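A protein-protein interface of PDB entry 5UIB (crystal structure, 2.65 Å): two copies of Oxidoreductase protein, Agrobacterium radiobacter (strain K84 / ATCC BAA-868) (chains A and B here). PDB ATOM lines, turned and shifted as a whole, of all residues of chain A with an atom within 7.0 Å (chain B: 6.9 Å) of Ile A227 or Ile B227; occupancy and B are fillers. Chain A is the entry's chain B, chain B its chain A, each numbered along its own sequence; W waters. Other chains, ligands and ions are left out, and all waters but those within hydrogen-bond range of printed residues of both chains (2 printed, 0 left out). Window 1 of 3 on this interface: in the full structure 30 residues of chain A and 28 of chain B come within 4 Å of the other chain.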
ATOM      1  N   TRP A 150       7.388  -0.100  -6.405  1.00  0.00           N
ATOM      2  CA  TRP A 150       6.084   0.197  -5.808  1.00  0.00           C
ATOM      3  C   TRP A 150       5.738  -0.831  -4.753  1.00  0.00           C
ATOM      4  O   TRP A 150       6.044  -2.004  -4.911  1.00  0.00           O
ATOM      5  CB  TRP A 150       4.984   0.233  -6.892  1.00  0.00           C
ATOM      6  CG  TRP A 150       3.622   0.713  -6.409  1.00  0.00           C
ATOM      7  CD1 TRP A 150       3.227   2.005  -6.255  1.00  0.00           C
ATOM      8  CD2 TRP A 150       2.500  -0.099  -6.018  1.00  0.00           C
ATOM      9  NE1 TRP A 150       1.938   2.052  -5.784  1.00  0.00           N
ATOM     10  CE2 TRP A 150       1.465   0.777  -5.639  1.00  0.00           C
ATOM     11  CE3 TRP A 150       2.272  -1.483  -5.961  1.00  0.00           C
ATOM     12  CZ2 TRP A 150       0.215   0.323  -5.203  1.00  0.00           C
ATOM     13  CZ3 TRP A 150       1.027  -1.936  -5.531  1.00  0.00           C
ATOM     14  CH2 TRP A 150       0.014  -1.031  -5.156  1.00  0.00           C
ATOM     15  N   GLY A 151       5.086  -0.390  -3.687  1.00  0.00           N
ATOM     16  CA  GLY A 151       4.666  -1.292  -2.646  1.00  0.00           C
ATOM     17  C   GLY A 151       3.307  -0.973  -2.065  1.00  0.00           C
ATOM     18  O   GLY A 151       2.853   0.166  -2.099  1.00  0.00           O
ATOM     19  N   ARG A 152       2.654  -2.006  -1.541  1.00  0.00           N
ATOM     20  CA  ARG A 152       1.489  -1.845  -0.689  1.00  0.00           C
ATOM     21  C   ARG A 152       1.656  -2.695   0.559  1.00  0.00           C
ATOM     22  O   ARG A 152       2.005  -3.873   0.472  1.00  0.00           O
ATOM     23  CB  ARG A 152       0.208  -2.258  -1.395  1.00  0.00           C
ATOM     24  CG  ARG A 152      -1.027  -1.741  -0.684  1.00  0.00           C
ATOM     25  CD  ARG A 152      -2.178  -2.718  -0.749  1.00  0.00           C
ATOM     26  NE  ARG A 152      -3.379  -2.179  -0.093  1.00  0.00           N
ATOM     27  CZ  ARG A 152      -4.528  -2.835   0.049  1.00  0.00           C
ATOM     28  NH1 ARG A 152      -4.667  -4.066  -0.432  1.00  0.00           N
ATOM     29  NH2 ARG A 152      -5.543  -2.261   0.684  1.00  0.00           N
ATOM     30  N   PHE A 153       1.374  -2.072   1.702  1.00  0.00           N
ATOM     31  CA  PHE A 153       1.440  -2.690   3.014  1.00  0.00           C
ATOM     32  C   PHE A 153       0.109  -2.439   3.742  1.00  0.00           C
ATOM     33  O   PHE A 153      -0.185  -1.323   4.144  1.00  0.00           O
ATOM     34  CB  PHE A 153       2.620  -2.099   3.782  1.00  0.00           C
ATOM     35  CG  PHE A 153       3.908  -2.143   3.019  1.00  0.00           C
ATOM     36  CD1 PHE A 153       4.729  -3.273   3.081  1.00  0.00           C
ATOM     37  CD2 PHE A 153       4.294  -1.074   2.213  1.00  0.00           C
ATOM     38  CE1 PHE A 153       5.914  -3.330   2.363  1.00  0.00           C
ATOM     39  CE2 PHE A 153       5.488  -1.129   1.500  1.00  0.00           C
ATOM     40  CZ  PHE A 153       6.295  -2.256   1.572  1.00  0.00           C
ATOM     41  N   SER A 154      -0.680  -3.495   3.914  1.00  0.00           N
ATOM     42  CA  SER A 154      -2.076  -3.384   4.290  1.00  0.00           C
ATOM     43  C   SER A 154      -2.364  -4.227   5.537  1.00  0.00           C
ATOM     44  O   SER A 154      -2.041  -5.411   5.561  1.00  0.00           O
ATOM     45  CB  SER A 154      -2.921  -3.865   3.105  1.00  0.00           C
ATOM     46  OG  SER A 154      -4.302  -3.782   3.368  1.00  0.00           O
ATOM     47  N   THR A 183       3.484  -1.306  10.494  1.00  0.00           N
ATOM     48  CA  THR A 183       3.339  -1.336   9.036  1.00  0.00           C
ATOM     49  C   THR A 183       4.274  -0.325   8.352  1.00  0.00           C
ATOM     50  O   THR A 183       4.730  -0.567   7.225  1.00  0.00           O
ATOM     51  CB  THR A 183       1.870  -1.086   8.619  1.00  0.00           C
ATOM     52  OG1 THR A 183       0.994  -1.717   9.563  1.00  0.00           O
ATOM     53  CG2 THR A 183       1.591  -1.634   7.215  1.00  0.00           C
ATOM     54  N   ALA A 187       7.463  -1.109   5.882  1.00  0.00           N
ATOM     55  CA  ALA A 187       7.679  -0.398   4.623  1.00  0.00           C
ATOM     56  C   ALA A 187       9.144   0.004   4.474  1.00  0.00           C
ATOM     57  O   ALA A 187       9.720  -0.134   3.393  1.00  0.00           O
ATOM     58  CB  ALA A 187       6.759   0.813   4.512  1.00  0.00           C
ATOM     59  N   LEU A 191      11.441  -1.608   1.651  1.00  0.00           N
ATOM     60  CA  LEU A 191      11.774  -0.619   0.601  1.00  0.00           C
ATOM     61  C   LEU A 191      12.750   0.504   0.995  1.00  0.00           C
ATOM     62  O   LEU A 191      13.045   1.390   0.200  1.00  0.00           O
ATOM     63  CB  LEU A 191      10.481  -0.010   0.038  1.00  0.00           C
ATOM     64  CG  LEU A 191       9.532  -0.971  -0.692  1.00  0.00           C
ATOM     65  CD1 LEU A 191       8.323  -0.211  -1.226  1.00  0.00           C
ATOM     66  CD2 LEU A 191      10.242  -1.733  -1.812  1.00  0.00           C
ATOM     67  N   THR A 215      -4.530   5.966   6.069  1.00  0.00           N
ATOM     68  CA  THR A 215      -4.061   5.696   4.719  1.00  0.00           C
ATOM     69  C   THR A 215      -2.884   6.624   4.500  1.00  0.00           C
ATOM     70  O   THR A 215      -3.060   7.842   4.495  1.00  0.00           O
ATOM     71  CB  THR A 215      -5.152   5.972   3.661  1.00  0.00           C
ATOM     72  OG1 THR A 215      -6.315   5.184   3.945  1.00  0.00           O
ATOM     73  CG2 THR A 215      -4.666   5.620   2.271  1.00  0.00           C
ATOM     74  N   ILE A 216      -1.699   6.038   4.322  1.00  0.00           N
ATOM     75  CA  ILE A 216      -0.437   6.770   4.264  1.00  0.00           C
ATOM     76  C   ILE A 216       0.242   6.465   2.932  1.00  0.00           C
ATOM     77  O   ILE A 216       0.290   5.315   2.511  1.00  0.00           O
ATOM     78  CB  ILE A 216       0.508   6.369   5.434  1.00  0.00           C
ATOM     79  CG1 ILE A 216      -0.185   6.544   6.796  1.00  0.00           C
ATOM     80  CG2 ILE A 216       1.798   7.185   5.397  1.00  0.00           C
ATOM     81  CD1 ILE A 216       0.553   5.926   7.966  1.00  0.00           C
ATOM     82  N   LEU A 217       0.768   7.505   2.289  1.00  0.00           N
ATOM     83  CA  LEU A 217       1.452   7.407   0.991  1.00  0.00           C
ATOM     84  C   LEU A 217       2.910   7.831   1.172  1.00  0.00           C
ATOM     85  O   LEU A 217       3.173   8.967   1.566  1.00  0.00           O
ATOM     86  CB  LEU A 217       0.761   8.322  -0.027  1.00  0.00           C
ATOM     87  CG  LEU A 217       1.501   8.628  -1.338  1.00  0.00           C
ATOM     88  CD1 LEU A 217       1.429   7.419  -2.247  1.00  0.00           C
ATOM     89  CD2 LEU A 217       0.934   9.860  -2.027  1.00  0.00           C
ATOM     90  N   LEU A 218       3.846   6.941   0.847  1.00  0.00           N
ATOM     91  CA  LEU A 218       5.263   7.133   1.171  1.00  0.00           C
ATOM     92  C   LEU A 218       6.122   7.307  -0.068  1.00  0.00           C
ATOM     93  O   LEU A 218       6.017   6.521  -1.011  1.00  0.00           O
ATOM     94  CB  LEU A 218       5.771   5.924   1.952  1.00  0.00           C
ATOM     95  CG  LEU A 218       4.977   5.592   3.213  1.00  0.00           C
ATOM     96  CD1 LEU A 218       5.427   4.254   3.771  1.00  0.00           C
ATOM     97  CD2 LEU A 218       5.127   6.704   4.244  1.00  0.00           C
ATOM     98  N   HIS A 220       9.814   6.880  -1.071  1.00  0.00           N
ATOM     99  CA  HIS A 220      11.075   6.284  -0.606  1.00  0.00           C
ATOM    100  C   HIS A 220      12.258   6.923  -1.312  1.00  0.00           C
ATOM    101  O   HIS A 220      12.156   7.304  -2.477  1.00  0.00           O
ATOM    102  CB  HIS A 220      11.088   4.765  -0.820  1.00  0.00           C
ATOM    103  CG  HIS A 220      10.042   4.036  -0.033  1.00  0.00           C
ATOM    104  ND1 HIS A 220      10.203   3.716   1.300  1.00  0.00           N
ATOM    105  CD2 HIS A 220       8.821   3.568  -0.388  1.00  0.00           C
ATOM    106  CE1 HIS A 220       9.126   3.081   1.731  1.00  0.00           C
ATOM    107  NE2 HIS A 220       8.270   2.984   0.728  1.00  0.00           N
ATOM    108  N   THR A 225       7.532   4.127  -4.402  1.00  0.00           N
ATOM    109  CA  THR A 225       6.342   4.691  -3.779  1.00  0.00           C
ATOM    110  C   THR A 225       5.641   3.571  -3.010  1.00  0.00           C
ATOM    111  O   THR A 225       5.713   2.415  -3.420  1.00  0.00           O
ATOM    112  CB  THR A 225       5.401   5.201  -4.875  1.00  0.00           C
ATOM    113  OG1 THR A 225       6.106   6.119  -5.714  1.00  0.00           O
ATOM    114  CG2 THR A 225       4.185   5.877  -4.281  1.00  0.00           C
ATOM    115  N   SER A 226       4.959   3.865  -1.908  1.00  0.00           N
ATOM    116  CA  SER A 226       4.098   2.823  -1.316  1.00  0.00           C
ATOM    117  C   SER A 226       2.893   3.332  -0.550  1.00  0.00           C
ATOM    118  O   SER A 226       2.843   4.490  -0.154  1.00  0.00           O
ATOM    119  CB  SER A 226       4.899   1.876  -0.419  1.00  0.00           C
ATOM    120  OG  SER A 226       5.244   2.493   0.809  1.00  0.00           O
ATOM    121  N   ILE A 227       1.933   2.437  -0.343  1.00  0.00           N
ATOM    122  CA  ILE A 227       0.724   2.750   0.405  1.00  0.00           C
ATOM    123  C   ILE A 227       0.751   1.931   1.679  1.00  0.00           C
ATOM    124  O   ILE A 227       0.851   0.714   1.620  1.00  0.00           O
ATOM    125  CB  ILE A 227      -0.572   2.424  -0.403  1.00  0.00           C
ATOM    126  CG1 ILE A 227      -0.524   3.029  -1.815  1.00  0.00           C
ATOM    127  CG2 ILE A 227      -1.825   2.918   0.323  1.00  0.00           C
ATOM    128  CD1 ILE A 227      -0.259   4.526  -1.852  1.00  0.00           C
ATOM    129  N   VAL A 228       0.699   2.599   2.826  1.00  0.00           N
ATOM    130  CA  VAL A 228       0.444   1.927   4.087  1.00  0.00           C
ATOM    131  C   VAL A 228      -0.987   2.271   4.413  1.00  0.00           C
ATOM    132  O   VAL A 228      -1.300   3.436   4.654  1.00  0.00           O
ATOM    133  CB  VAL A 228       1.398   2.370   5.224  1.00  0.00           C
ATOM    134  CG1 VAL A 228       0.973   1.772   6.562  1.00  0.00           C
ATOM    135  CG2 VAL A 228       2.833   1.968   4.899  1.00  0.00           C
ATOM    136  N   ASP A 229      -1.855   1.263   4.378  1.00  0.00           N
ATOM    137  CA  ASP A 229      -3.258   1.420   4.749  1.00  0.00           C
ATOM    138  C   ASP A 229      -3.607   0.464   5.893  1.00  0.00           C
ATOM    139  O   ASP A 229      -3.417  -0.747   5.790  1.00  0.00           O
ATOM    140  CB  ASP A 229      -4.179   1.204   3.547  1.00  0.00           C
ATOM    141  CG  ASP A 229      -4.165  -0.220   3.046  1.00  0.00           C
ATOM    142  OD1 ASP A 229      -3.060  -0.728   2.749  1.00  0.00           O
ATOM    143  OD2 ASP A 229      -5.256  -0.830   2.961  1.00  0.00           O
ATOM    144  N   LEU A 245      -0.688  -7.918   4.775  1.00  0.00           N
ATOM    145  CA  LEU A 245      -0.719  -8.297   3.356  1.00  0.00           C
ATOM    146  C   LEU A 245       0.179  -7.354   2.561  1.00  0.00           C
ATOM    147  O   LEU A 245      -0.012  -6.142   2.606  1.00  0.00           O
ATOM    148  CB  LEU A 245      -2.156  -8.226   2.830  1.00  0.00           C
ATOM    149  CG  LEU A 245      -3.179  -8.992   3.680  1.00  0.00           C
ATOM    150  CD1 LEU A 245      -4.568  -8.897   3.078  1.00  0.00           C
ATOM    151  CD2 LEU A 245      -2.765 -10.446   3.851  1.00  0.00           C
ATOM    152  N   TRP B 150     -13.821   4.227   3.015  1.00  0.00           N
ATOM    153  CA  TRP B 150     -12.503   4.029   2.428  1.00  0.00           C
ATOM    154  C   TRP B 150     -12.631   3.191   1.175  1.00  0.00           C
ATOM    155  O   TRP B 150     -13.425   2.255   1.141  1.00  0.00           O
ATOM    156  CB  TRP B 150     -11.559   3.345   3.433  1.00  0.00           C
ATOM    157  CG  TRP B 150     -10.175   3.084   2.892  1.00  0.00           C
ATOM    158  CD1 TRP B 150      -9.097   3.932   2.930  1.00  0.00           C
ATOM    159  CD2 TRP B 150      -9.731   1.899   2.217  1.00  0.00           C
ATOM    160  NE1 TRP B 150      -8.009   3.346   2.318  1.00  0.00           N
ATOM    161  CE2 TRP B 150      -8.366   2.099   1.874  1.00  0.00           C
ATOM    162  CE3 TRP B 150     -10.352   0.683   1.871  1.00  0.00           C
ATOM    163  CZ2 TRP B 150      -7.604   1.122   1.203  1.00  0.00           C
ATOM    164  CZ3 TRP B 150      -9.596  -0.290   1.201  1.00  0.00           C
ATOM    165  CH2 TRP B 150      -8.233  -0.062   0.877  1.00  0.00           C
ATOM    166  N   GLY B 151     -11.835   3.509   0.159  1.00  0.00           N
ATOM    167  CA  GLY B 151     -11.842   2.752  -1.095  1.00  0.00           C
ATOM    168  C   GLY B 151     -10.476   2.531  -1.732  1.00  0.00           C
ATOM    169  O   GLY B 151      -9.501   3.222  -1.420  1.00  0.00           O
ATOM    170  N   ARG B 152     -10.409   1.551  -2.627  1.00  0.00           N
ATOM    171  CA  ARG B 152      -9.233   1.347  -3.451  1.00  0.00           C
ATOM    172  C   ARG B 152      -9.648   0.891  -4.829  1.00  0.00           C
ATOM    173  O   ARG B 152     -10.480  -0.003  -4.955  1.00  0.00           O
ATOM    174  CB  ARG B 152      -8.323   0.297  -2.844  1.00  0.00           C
ATOM    175  CG  ARG B 152      -6.999   0.163  -3.577  1.00  0.00           C
ATOM    176  CD  ARG B 152      -6.458  -1.252  -3.552  1.00  0.00           C
ATOM    177  NE  ARG B 152      -5.303  -1.366  -4.439  1.00  0.00           N
ATOM    178  CZ  ARG B 152      -4.364  -2.302  -4.356  1.00  0.00           C
ATOM    179  NH1 ARG B 152      -4.420  -3.242  -3.418  1.00  0.00           N
ATOM    180  NH2 ARG B 152      -3.357  -2.299  -5.226  1.00  0.00           N
ATOM    181  N   PHE B 153      -9.030   1.499  -5.841  1.00  0.00           N
ATOM    182  CA  PHE B 153      -9.291   1.205  -7.247  1.00  0.00           C
ATOM    183  C   PHE B 153      -7.954   0.920  -7.935  1.00  0.00           C
ATOM    184  O   PHE B 153      -7.076   1.776  -7.945  1.00  0.00           O
ATOM    185  CB  PHE B 153     -10.028   2.390  -7.907  1.00  0.00           C
ATOM    186  CG  PHE B 153     -11.292   2.788  -7.183  1.00  0.00           C
ATOM    187  CD1 PHE B 153     -11.245   3.667  -6.094  1.00  0.00           C
ATOM    188  CD2 PHE B 153     -12.523   2.262  -7.561  1.00  0.00           C
ATOM    189  CE1 PHE B 153     -12.399   4.016  -5.412  1.00  0.00           C
ATOM    190  CE2 PHE B 153     -13.681   2.608  -6.878  1.00  0.00           C
ATOM    191  CZ  PHE B 153     -13.618   3.484  -5.801  1.00  0.00           C
ATOM    192  N   SER B 154      -7.807  -0.279  -8.501  1.00  0.00           N
ATOM    193  CA  SER B 154      -6.513  -0.770  -9.007  1.00  0.00           C
ATOM    194  C   SER B 154      -6.614  -1.301 -10.454  1.00  0.00           C
ATOM    195  O   SER B 154      -7.505  -2.089 -10.782  1.00  0.00           O
ATOM    196  CB  SER B 154      -5.967  -1.861  -8.068  1.00  0.00           C
ATOM    197  OG  SER B 154      -4.552  -1.915  -8.074  1.00  0.00           O
ATOM    198  N   THR B 183     -10.093   5.043 -14.155  1.00  0.00           N
ATOM    199  CA  THR B 183     -10.024   4.610 -12.752  1.00  0.00           C
ATOM    200  C   THR B 183     -10.444   5.750 -11.807  1.00  0.00           C
ATOM    201  O   THR B 183     -11.131   5.515 -10.800  1.00  0.00           O
ATOM    202  CB  THR B 183      -8.614   4.083 -12.389  1.00  0.00           C
ATOM    203  OG1 THR B 183      -8.106   3.279 -13.457  1.00  0.00           O
ATOM    204  CG2 THR B 183      -8.644   3.246 -11.104  1.00  0.00           C
ATOM    205  N   ALA B 187     -13.746   6.065  -9.283  1.00  0.00           N
ATOM    206  CA  ALA B 187     -13.651   6.518  -7.886  1.00  0.00           C
ATOM    207  C   ALA B 187     -14.721   7.552  -7.584  1.00  0.00           C
ATOM    208  O   ALA B 187     -15.380   7.485  -6.547  1.00  0.00           O
ATOM    209  CB  ALA B 187     -12.264   7.066  -7.583  1.00  0.00           C
ATOM    210  N   LEU B 191     -17.703   6.666  -5.099  1.00  0.00           N
ATOM    211  CA  LEU B 191     -17.591   7.406  -3.812  1.00  0.00           C
ATOM    212  C   LEU B 191     -17.859   8.934  -3.828  1.00  0.00           C
ATOM    213  O   LEU B 191     -17.742   9.591  -2.780  1.00  0.00           O
ATOM    214  CB  LEU B 191     -16.216   7.126  -3.178  1.00  0.00           C
ATOM    215  CG  LEU B 191     -15.877   5.663  -2.869  1.00  0.00           C
ATOM    216  CD1 LEU B 191     -14.568   5.595  -2.097  1.00  0.00           C
ATOM    217  CD2 LEU B 191     -16.981   4.976  -2.078  1.00  0.00           C
ATOM    218  N   THR B 215       0.179   6.609  -8.657  1.00  0.00           N
ATOM    219  CA  THR B 215      -0.496   6.320  -7.406  1.00  0.00           C
ATOM    220  C   THR B 215      -1.098   7.599  -6.887  1.00  0.00           C
ATOM    221  O   THR B 215      -0.389   8.545  -6.617  1.00  0.00           O
ATOM    222  CB  THR B 215       0.487   5.780  -6.368  1.00  0.00           C
ATOM    223  OG1 THR B 215       1.059   4.568  -6.861  1.00  0.00           O
ATOM    224  CG2 THR B 215      -0.201   5.501  -5.046  1.00  0.00           C
ATOM    225  N   ILE B 216      -2.412   7.602  -6.736  1.00  0.00           N
ATOM    226  CA  ILE B 216      -3.173   8.808  -6.467  1.00  0.00           C
ATOM    227  C   ILE B 216      -4.007   8.552  -5.207  1.00  0.00           C
ATOM    228  O   ILE B 216      -4.598   7.476  -5.052  1.00  0.00           O
ATOM    229  CB  ILE B 216      -4.056   9.177  -7.688  1.00  0.00           C
ATOM    230  CG1 ILE B 216      -3.211   9.212  -8.973  1.00  0.00           C
ATOM    231  CG2 ILE B 216      -4.719  10.532  -7.499  1.00  0.00           C
ATOM    232  CD1 ILE B 216      -3.987   9.533 -10.230  1.00  0.00           C
ATOM    233  N   LEU B 217      -4.026   9.545  -4.314  1.00  0.00           N
ATOM    234  CA  LEU B 217      -4.701   9.474  -3.010  1.00  0.00           C
ATOM    235  C   LEU B 217      -5.761  10.562  -2.978  1.00  0.00           C
ATOM    236  O   LEU B 217      -5.442  11.736  -3.123  1.00  0.00           O
ATOM    237  CB  LEU B 217      -3.681   9.697  -1.890  1.00  0.00           C
ATOM    238  CG  LEU B 217      -4.169   9.867  -0.447  1.00  0.00           C
ATOM    239  CD1 LEU B 217      -4.399   8.500   0.175  1.00  0.00           C
ATOM    240  CD2 LEU B 217      -3.187  10.685   0.381  1.00  0.00           C
ATOM    241  N   LEU B 218      -7.010  10.168  -2.762  1.00  0.00           N
ATOM    242  CA  LEU B 218      -8.156  11.035  -2.999  1.00  0.00           C
ATOM    243  C   LEU B 218      -8.929  11.311  -1.715  1.00  0.00           C
ATOM    244  O   LEU B 218      -9.287  10.388  -0.993  1.00  0.00           O
ATOM    245  CB  LEU B 218      -9.076  10.369  -4.024  1.00  0.00           C
ATOM    246  CG  LEU B 218      -8.459   9.990  -5.380  1.00  0.00           C
ATOM    247  CD1 LEU B 218      -9.483   9.345  -6.303  1.00  0.00           C
ATOM    248  CD2 LEU B 218      -7.863  11.223  -6.048  1.00  0.00           C
ATOM    249  N   HIS B 220     -12.418  12.408  -0.710  1.00  0.00           N
ATOM    250  CA  HIS B 220     -13.771  12.626  -1.232  1.00  0.00           C
ATOM    251  C   HIS B 220     -14.556  13.645  -0.388  1.00  0.00           C
ATOM    252  O   HIS B 220     -14.436  13.677   0.843  1.00  0.00           O
ATOM    253  CB  HIS B 220     -14.523  11.300  -1.382  1.00  0.00           C
ATOM    254  CG  HIS B 220     -13.923  10.392  -2.410  1.00  0.00           C
ATOM    255  ND1 HIS B 220     -14.115  10.573  -3.763  1.00  0.00           N
ATOM    256  CD2 HIS B 220     -13.115   9.311  -2.287  1.00  0.00           C
ATOM    257  CE1 HIS B 220     -13.457   9.639  -4.429  1.00  0.00           C
ATOM    258  NE2 HIS B 220     -12.843   8.860  -3.557  1.00  0.00           N
ATOM    259  N   THR B 225     -11.877   8.360   2.083  1.00  0.00           N
ATOM    260  CA  THR B 225     -10.545   8.366   1.492  1.00  0.00           C
ATOM    261  C   THR B 225     -10.512   7.250   0.445  1.00  0.00           C
ATOM    262  O   THR B 225     -11.092   6.185   0.664  1.00  0.00           O
ATOM    263  CB  THR B 225      -9.471   8.094   2.577  1.00  0.00           C
ATOM    264  OG1 THR B 225      -9.486   9.146   3.553  1.00  0.00           O
ATOM    265  CG2 THR B 225      -8.070   7.989   1.977  1.00  0.00           C
ATOM    266  N   SER B 226      -9.850   7.480  -0.689  1.00  0.00           N
ATOM    267  CA  SER B 226      -9.635   6.395  -1.663  1.00  0.00           C
ATOM    268  C   SER B 226      -8.225   6.392  -2.254  1.00  0.00           C
ATOM    269  O   SER B 226      -7.548   7.415  -2.254  1.00  0.00           O
ATOM    270  CB  SER B 226     -10.687   6.434  -2.779  1.00  0.00           C
ATOM    271  OG  SER B 226     -10.255   7.215  -3.876  1.00  0.00           O
ATOM    272  N   ILE B 227      -7.814   5.223  -2.753  1.00  0.00           N
ATOM    273  CA  ILE B 227      -6.521   5.020  -3.415  1.00  0.00           C
ATOM    274  C   ILE B 227      -6.797   4.603  -4.848  1.00  0.00           C
ATOM    275  O   ILE B 227      -7.430   3.583  -5.072  1.00  0.00           O
ATOM    276  CB  ILE B 227      -5.694   3.897  -2.720  1.00  0.00           C
ATOM    277  CG1 ILE B 227      -5.287   4.302  -1.301  1.00  0.00           C
ATOM    278  CG2 ILE B 227      -4.435   3.535  -3.511  1.00  0.00           C
ATOM    279  CD1 ILE B 227      -4.173   5.333  -1.236  1.00  0.00           C
ATOM    280  N   VAL B 228      -6.337   5.397  -5.809  1.00  0.00           N
ATOM    281  CA  VAL B 228      -6.283   4.980  -7.209  1.00  0.00           C
ATOM    282  C   VAL B 228      -4.828   4.639  -7.509  1.00  0.00           C
ATOM    283  O   VAL B 228      -3.959   5.497  -7.373  1.00  0.00           O
ATOM    284  CB  VAL B 228      -6.753   6.096  -8.168  1.00  0.00           C
ATOM    285  CG1 VAL B 228      -6.657   5.648  -9.625  1.00  0.00           C
ATOM    286  CG2 VAL B 228      -8.168   6.527  -7.826  1.00  0.00           C
ATOM    287  N   ASP B 229      -4.546   3.400  -7.893  1.00  0.00           N
ATOM    288  CA  ASP B 229      -3.188   3.007  -8.246  1.00  0.00           C
ATOM    289  C   ASP B 229      -3.189   2.292  -9.586  1.00  0.00           C
ATOM    290  O   ASP B 229      -3.897   1.314  -9.764  1.00  0.00           O
ATOM    291  CB  ASP B 229      -2.542   2.159  -7.140  1.00  0.00           C
ATOM    292  CG  ASP B 229      -3.301   0.872  -6.841  1.00  0.00           C
ATOM    293  OD1 ASP B 229      -4.409   0.928  -6.268  1.00  0.00           O
ATOM    294  OD2 ASP B 229      -2.774  -0.214  -7.163  1.00  0.00           O
ATOM    295  N   LEU B 245      -9.759  -3.683 -10.281  1.00  0.00           N
ATOM    296  CA  LEU B 245     -10.003  -4.293  -8.969  1.00  0.00           C
ATOM    297  C   LEU B 245     -10.339  -3.236  -7.919  1.00  0.00           C
ATOM    298  O   LEU B 245      -9.689  -2.198  -7.848  1.00  0.00           O
ATOM    299  CB  LEU B 245      -8.769  -5.068  -8.504  1.00  0.00           C
ATOM    300  CG  LEU B 245      -8.166  -6.178  -9.378  1.00  0.00           C
ATOM    301  CD1 LEU B 245      -7.622  -7.264  -8.459  1.00  0.00           C
ATOM    302  CD2 LEU B 245      -9.150  -6.791 -10.363  1.00  0.00           C
HETATM  303  O   HOH W   1      -6.851   2.789   5.533  1.00  0.00           O
HETATM  304  O   HOH W   2       0.571   2.656  -8.884  1.00  0.00           O
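The backbone carbonyl oxygen (O) of Phe A153 is in hydrogen-bond range of the backbone NH (N) of Asp A229 (3.1 Å). The backbone carbonyl oxygen (O) of Gly A151 lies within hydrogen-bond range of the backbone NH (N) of Ile A227 (3.0 Å). The side-chain hydroxyl (OG) of Ser B154 lies within hydrogen-bond range of the guanidinium group (NH2) of Arg B152 (3.1 Å). The guanidinium group of Arg A152 is in salt-bridge range of the side-chain carboxylate of Asp A229, at 2.7 Å. OG of Ser A154 lies within hydrogen-bond range of NH2 of Arg A152. The side-chain hydroxyl of Ser B154 sits at hydrogen-bond distance from the side-chain carboxylate of Asp B229.
Water W2 lies within hydrogen-bond range of the side-chain hydroxyl (OG1) of Thr B215 and the indole nitrogen (NE1) of Trp A150. Water W1 bridges OG1 of Thr A215 and NE1 of Trp B150.
The guanidinium group (NH1) of Arg A152 sits close to the guanidinium group (NH1) of Arg B152 (3.1 Å). The indole nitrogen (NE1) of Trp B150 is in hydrogen-bond range of the side-chain hydroxyl (OG1) of Thr A215, at 3.0 Å. The indole nitrogen (NE1) of Trp A150 sits at hydrogen-bond distance from the side-chain hydroxyl (OG1) of Thr B215, 2.9 Å away.
Ile A227 touches just these residues of chain B: Thr B215 and Ile B227. Of chain A, only Thr A215 (3.6 Å) and Ile A227 (3.7 Å) come within 4 Å of Ile B227. Of the printed residues of chain A, Trp B150 touches Arg A152 (3.5 Å), Thr A215 (3.0 Å) and Asp A229 (3.5 Å). Printed residues of chain B within 4 Å of Thr A215: Trp B150 (3.0 Å), Leu B217 (3.6 Å), Thr B225 (3.8 Å) and Ile B227 (3.6 Å). Printed residues of chain B within 4 Å of Asp A229: Trp B150. Of the printed residues of chain B, Leu A217 touches Thr B215. Of the printed residues of chain A, Thr B215 touches Trp A150, Leu A217 and Ile A227. His B220 touches none of the printed residues of chain A. Val B228 touches none of the printed residues of chain A. The nearest residue of chain B that does not touch Ile A227 is Asp B229 (5.8 Å).
Among the printed residues, pairs that only touch across the chains: Ile A227 with Thr B215 (3.3 Å), Arg A152 with Trp B150 (3.5 Å), Asp A229 with Trp B150 (3.5 Å), Trp A150 with Asp B229 (3.5 Å), Thr A215 with Ile B227 (3.6 Å), Thr A215 with Leu B217 (3.6 Å), Trp A150 with Arg B152 (3.6 Å), Ile A227 with Ile B227 (3.7 Å), Leu A217 with Thr B215 (3.8 Å) and Thr A215 with Thr B225 (3.8 Å).
Hydrophobic or aromatic side chains of chain B that line the printed part of chain A: Trp B150, Leu B217 and Ile B227. Of the 19 printed residues of chain A, 6 touch a printed residue of chain B. Hydrophobic or aromatic side chains of chain A that line the printed part of chain B: Trp A150, Leu A217 and Ile A227. Among the printed residues, no Asp or Glu carboxylate lies within 4 Å of a Lys or Arg side-chain nitrogen of the other chain.
Trp A150 touches Thr B215, and with the chains exchanged Thr A215 touches Trp B150. Thr A215 touches Leu B217, and with the chains exchanged Leu A217 touches Thr B215. Thr A215 touches Ile B227, and with the chains exchanged Ile A227 touches Thr B215. Ile B227 touches its own counterpart, Ile A227. Positions printed for both chains: 150, 151, 152, 153, 154, 183, 187, 191, 215, 216, 217, 218, 220, 225, 226, 227, 228, 229 and 245.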
